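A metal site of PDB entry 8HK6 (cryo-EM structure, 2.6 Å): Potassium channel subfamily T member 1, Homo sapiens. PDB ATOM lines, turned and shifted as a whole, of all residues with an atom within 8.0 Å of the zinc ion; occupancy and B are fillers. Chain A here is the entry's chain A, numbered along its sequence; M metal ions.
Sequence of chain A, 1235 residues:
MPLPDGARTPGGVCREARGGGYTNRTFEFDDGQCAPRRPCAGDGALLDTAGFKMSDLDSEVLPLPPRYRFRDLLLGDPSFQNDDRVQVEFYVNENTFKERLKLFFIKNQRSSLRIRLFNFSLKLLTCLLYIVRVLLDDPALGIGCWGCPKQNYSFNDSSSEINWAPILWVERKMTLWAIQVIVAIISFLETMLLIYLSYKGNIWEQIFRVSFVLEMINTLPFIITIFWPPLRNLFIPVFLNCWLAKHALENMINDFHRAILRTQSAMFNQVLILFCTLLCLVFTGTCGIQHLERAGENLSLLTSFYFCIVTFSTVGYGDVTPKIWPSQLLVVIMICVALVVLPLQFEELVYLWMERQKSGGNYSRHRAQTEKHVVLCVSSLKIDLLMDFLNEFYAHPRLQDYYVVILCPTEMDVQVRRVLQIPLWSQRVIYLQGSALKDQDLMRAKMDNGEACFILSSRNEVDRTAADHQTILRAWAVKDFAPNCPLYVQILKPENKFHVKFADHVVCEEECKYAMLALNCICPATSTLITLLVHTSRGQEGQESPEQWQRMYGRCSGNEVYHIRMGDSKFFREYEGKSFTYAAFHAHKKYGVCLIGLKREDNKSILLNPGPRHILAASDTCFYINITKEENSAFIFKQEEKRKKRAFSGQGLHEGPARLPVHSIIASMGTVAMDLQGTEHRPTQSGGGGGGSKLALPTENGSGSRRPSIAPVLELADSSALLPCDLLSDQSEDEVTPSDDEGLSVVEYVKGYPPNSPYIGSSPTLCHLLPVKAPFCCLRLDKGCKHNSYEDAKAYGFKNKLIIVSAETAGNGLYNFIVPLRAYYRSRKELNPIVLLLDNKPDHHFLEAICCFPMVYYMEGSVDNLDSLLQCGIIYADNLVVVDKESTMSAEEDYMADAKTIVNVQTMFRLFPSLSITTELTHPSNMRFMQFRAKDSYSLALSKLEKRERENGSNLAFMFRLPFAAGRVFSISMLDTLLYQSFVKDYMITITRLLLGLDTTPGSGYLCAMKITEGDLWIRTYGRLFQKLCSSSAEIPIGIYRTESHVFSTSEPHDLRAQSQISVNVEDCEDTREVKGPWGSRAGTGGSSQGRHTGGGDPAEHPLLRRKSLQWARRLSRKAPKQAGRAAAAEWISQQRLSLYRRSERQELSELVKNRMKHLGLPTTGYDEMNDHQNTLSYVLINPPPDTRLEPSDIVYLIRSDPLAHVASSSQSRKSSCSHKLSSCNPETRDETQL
The zinc ion is bound by ND1 of His 787, at 2.1 Å. The zinc ion is bound by SG of Cys 777 (2.3 Å). SG of Cys 785 binds the zinc ion, at 2.3 Å. SG of Cys 778 is bound to the zinc ion, 2.3 Å away. The zinc ion has four donor atoms within binding distance.
Within 4 Å of the zinc ion: Cys 777, Cys 778, Cys 785 and His 787.
SG of Cys 785 lies close to OD1 of Asn 788, at 3.0 Å.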
ATOM      1  N   ALA A 774       6.991  19.180 -12.806  1.00  0.00           N
ATOM      2  CA  ALA A 774       8.278  19.550 -12.225  1.00  0.00           C
ATOM      3  C   ALA A 774       9.292  18.451 -12.473  1.00  0.00           C
ATOM      4  O   ALA A 774       9.020  17.275 -12.159  1.00  0.00           O
ATOM      5  CB  ALA A 774       8.133  19.795 -10.725  1.00  0.00           C
ATOM      6  N   PRO A 775      10.457  18.762 -13.034  1.00  0.00           N
ATOM      7  CA  PRO A 775      11.501  17.747 -13.181  1.00  0.00           C
ATOM      8  C   PRO A 775      11.936  17.212 -11.822  1.00  0.00           C
ATOM      9  O   PRO A 775      11.891  17.909 -10.810  1.00  0.00           O
ATOM     10  CB  PRO A 775      12.640  18.504 -13.879  1.00  0.00           C
ATOM     11  CG  PRO A 775      12.298  19.949 -13.754  1.00  0.00           C
ATOM     12  CD  PRO A 775      10.813  20.029 -13.697  1.00  0.00           C
ATOM     13  N   PHE A 776      12.335  15.935 -11.811  1.00  0.00           N
ATOM     14  CA  PHE A 776      12.623  15.248 -10.563  1.00  0.00           C
ATOM     15  C   PHE A 776      13.732  15.911  -9.770  1.00  0.00           C
ATOM     16  O   PHE A 776      13.759  15.790  -8.539  1.00  0.00           O
ATOM     17  CB  PHE A 776      13.002  13.787 -10.846  1.00  0.00           C
ATOM     18  CG  PHE A 776      11.871  12.947 -11.353  1.00  0.00           C
ATOM     19  CD1 PHE A 776      10.632  13.492 -11.615  1.00  0.00           C
ATOM     20  CD2 PHE A 776      12.054  11.590 -11.564  1.00  0.00           C
ATOM     21  CE1 PHE A 776       9.599  12.718 -12.080  1.00  0.00           C
ATOM     22  CE2 PHE A 776      11.014  10.814 -12.036  1.00  0.00           C
ATOM     23  CZ  PHE A 776       9.793  11.382 -12.294  1.00  0.00           C
ATOM     24  N   CYS A 777      14.649  16.613 -10.436  1.00  0.00           N
ATOM     25  CA  CYS A 777      15.688  17.347  -9.723  1.00  0.00           C
ATOM     26  C   CYS A 777      15.100  18.498  -8.920  1.00  0.00           C
ATOM     27  O   CYS A 777      15.622  18.843  -7.851  1.00  0.00           O
ATOM     28  CB  CYS A 777      16.727  17.874 -10.709  1.00  0.00           C
ATOM     29  SG  CYS A 777      16.091  19.095 -11.882  1.00  0.00           S
ATOM     30  N   CYS A 778      14.016  19.096  -9.404  1.00  0.00           N
ATOM     31  CA  CYS A 778      13.414  20.226  -8.708  1.00  0.00           C
ATOM     32  C   CYS A 778      12.570  19.788  -7.525  1.00  0.00           C
ATOM     33  O   CYS A 778      12.170  20.630  -6.710  1.00  0.00           O
ATOM     34  CB  CYS A 778      12.573  21.058  -9.680  1.00  0.00           C
ATOM     35  SG  CYS A 778      13.555  21.864 -10.965  1.00  0.00           S
ATOM     36  N   LEU A 779      12.292  18.486  -7.394  1.00  0.00           N
ATOM     37  CA  LEU A 779      11.592  17.968  -6.239  1.00  0.00           C
ATOM     38  C   LEU A 779      12.520  17.631  -5.088  1.00  0.00           C
ATOM     39  O   LEU A 779      12.037  17.192  -4.038  1.00  0.00           O
ATOM     40  CB  LEU A 779      10.798  16.706  -6.632  1.00  0.00           C
ATOM     41  CG  LEU A 779       9.861  16.821  -7.824  1.00  0.00           C
ATOM     42  CD1 LEU A 779       9.145  15.496  -8.045  1.00  0.00           C
ATOM     43  CD2 LEU A 779       8.866  17.934  -7.611  1.00  0.00           C
ATOM     44  N   ARG A 780      13.824  17.823  -5.249  1.00  0.00           N
ATOM     45  CA  ARG A 780      14.784  17.498  -4.202  1.00  0.00           C
ATOM     46  C   ARG A 780      15.211  18.768  -3.473  1.00  0.00           C
ATOM     47  O   ARG A 780      15.813  19.660  -4.078  1.00  0.00           O
ATOM     48  CB  ARG A 780      16.003  16.772  -4.775  1.00  0.00           C
ATOM     49  CG  ARG A 780      16.879  16.181  -3.695  1.00  0.00           C
ATOM     50  CD  ARG A 780      17.405  14.826  -4.080  1.00  0.00           C
ATOM     51  NE  ARG A 780      18.789  14.657  -3.658  1.00  0.00           N
ATOM     52  CZ  ARG A 780      19.185  13.894  -2.648  1.00  0.00           C
ATOM     53  NH1 ARG A 780      18.312  13.210  -1.916  1.00  0.00           N
ATOM     54  NH2 ARG A 780      20.480  13.827  -2.355  1.00  0.00           N
ATOM     55  N   LYS A 783      19.808  18.625  -2.998  1.00  0.00           N
ATOM     56  CA  LYS A 783      20.761  19.005  -4.028  1.00  0.00           C
ATOM     57  C   LYS A 783      20.233  20.157  -4.857  1.00  0.00           C
ATOM     58  O   LYS A 783      19.047  20.208  -5.208  1.00  0.00           O
ATOM     59  CB  LYS A 783      21.084  17.822  -4.936  1.00  0.00           C
ATOM     60  CG  LYS A 783      21.489  16.557  -4.210  1.00  0.00           C
ATOM     61  CD  LYS A 783      21.474  15.355  -5.157  1.00  0.00           C
ATOM     62  CE  LYS A 783      21.952  15.716  -6.547  1.00  0.00           C
ATOM     63  NZ  LYS A 783      23.346  15.262  -6.801  1.00  0.00           N
ATOM     64  N   GLY A 784      21.128  21.079  -5.199  1.00  0.00           N
ATOM     65  CA  GLY A 784      20.804  22.097  -6.169  1.00  0.00           C
ATOM     66  C   GLY A 784      20.844  21.549  -7.577  1.00  0.00           C
ATOM     67  O   GLY A 784      21.529  20.567  -7.871  1.00  0.00           O
ATOM     68  N   CYS A 785      20.100  22.196  -8.459  1.00  0.00           N
ATOM     69  CA  CYS A 785      20.032  21.728  -9.843  1.00  0.00           C
ATOM     70  C   CYS A 785      20.251  22.856 -10.831  1.00  0.00           C
ATOM     71  O   CYS A 785      20.712  23.942 -10.463  1.00  0.00           O
ATOM     72  CB  CYS A 785      18.680  21.053 -10.116  1.00  0.00           C
ATOM     73  SG  CYS A 785      17.229  22.056  -9.758  1.00  0.00           S
ATOM     74  N   LYS A 786      19.962  22.588 -12.105  1.00  0.00           N
ATOM     75  CA  LYS A 786      20.124  23.591 -13.142  1.00  0.00           C
ATOM     76  C   LYS A 786      19.184  24.772 -12.903  1.00  0.00           C
ATOM     77  O   LYS A 786      19.572  25.929 -13.053  1.00  0.00           O
ATOM     78  CB  LYS A 786      19.858  22.987 -14.536  1.00  0.00           C
ATOM     79  CG  LYS A 786      20.038  23.870 -15.795  1.00  0.00           C
ATOM     80  CD  LYS A 786      19.819  23.247 -17.187  1.00  0.00           C
ATOM     81  CE  LYS A 786      20.013  24.262 -18.329  1.00  0.00           C
ATOM     82  NZ  LYS A 786      19.798  23.669 -19.691  1.00  0.00           N
ATOM     83  N   HIS A 787      17.940  24.477 -12.527  1.00  0.00           N
ATOM     84  CA  HIS A 787      16.937  25.518 -12.341  1.00  0.00           C
ATOM     85  C   HIS A 787      17.130  26.285 -11.038  1.00  0.00           C
ATOM     86  O   HIS A 787      16.728  27.446 -10.955  1.00  0.00           O
ATOM     87  CB  HIS A 787      15.530  24.906 -12.380  1.00  0.00           C
ATOM     88  CG  HIS A 787      15.393  23.770 -13.357  1.00  0.00           C
ATOM     89  ND1 HIS A 787      15.910  22.518 -13.126  1.00  0.00           N
ATOM     90  CD2 HIS A 787      14.800  23.714 -14.572  1.00  0.00           C
ATOM     91  CE1 HIS A 787      15.644  21.736 -14.156  1.00  0.00           C
ATOM     92  NE2 HIS A 787      14.968  22.435 -15.048  1.00  0.00           N
ATOM     93  N   ASN A 788      17.728  25.664 -10.023  1.00  0.00           N
ATOM     94  CA  ASN A 788      17.881  26.303  -8.729  1.00  0.00           C
ATOM     95  C   ASN A 788      19.117  25.766  -8.026  1.00  0.00           C
ATOM     96  O   ASN A 788      19.485  24.598  -8.187  1.00  0.00           O
ATOM     97  CB  ASN A 788      16.602  26.123  -7.885  1.00  0.00           C
ATOM     98  CG  ASN A 788      16.293  24.663  -7.535  1.00  0.00           C
ATOM     99  OD1 ASN A 788      17.190  23.846  -7.331  1.00  0.00           O
ATOM    100  ND2 ASN A 788      15.020  24.323  -7.501  1.00  0.00           N
ATOM    101  N   SER A 789      19.790  26.642  -7.288  1.00  0.00           N
ATOM    102  CA  SER A 789      20.960  26.269  -6.500  1.00  0.00           C
ATOM    103  C   SER A 789      20.636  26.053  -5.031  1.00  0.00           C
ATOM    104  O   SER A 789      21.542  25.800  -4.238  1.00  0.00           O
ATOM    105  CB  SER A 789      22.051  27.327  -6.630  1.00  0.00           C
ATOM    106  OG  SER A 789      21.639  28.565  -6.065  1.00  0.00           O
ATOM    107  N   TYR A 796      15.179  28.529  -0.196  1.00  0.00           N
ATOM    108  CA  TYR A 796      13.925  28.608  -0.945  1.00  0.00           C
ATOM    109  C   TYR A 796      13.152  29.863  -0.590  1.00  0.00           C
ATOM    110  O   TYR A 796      12.599  30.532  -1.478  1.00  0.00           O
ATOM    111  CB  TYR A 796      13.082  27.368  -0.686  1.00  0.00           C
ATOM    112  CG  TYR A 796      13.457  26.165  -1.511  1.00  0.00           C
ATOM    113  CD1 TYR A 796      14.581  25.425  -1.221  1.00  0.00           C
ATOM    114  CD2 TYR A 796      12.688  25.781  -2.601  1.00  0.00           C
ATOM    115  CE1 TYR A 796      14.930  24.328  -1.968  1.00  0.00           C
ATOM    116  CE2 TYR A 796      13.029  24.686  -3.368  1.00  0.00           C
ATOM    117  CZ  TYR A 796      14.151  23.969  -3.041  1.00  0.00           C
ATOM    118  OH  TYR A 796      14.494  22.870  -3.795  1.00  0.00           O
HETATM  119 ZN    ZN M   1      15.775  21.337 -11.409  1.00  0.00          ZN
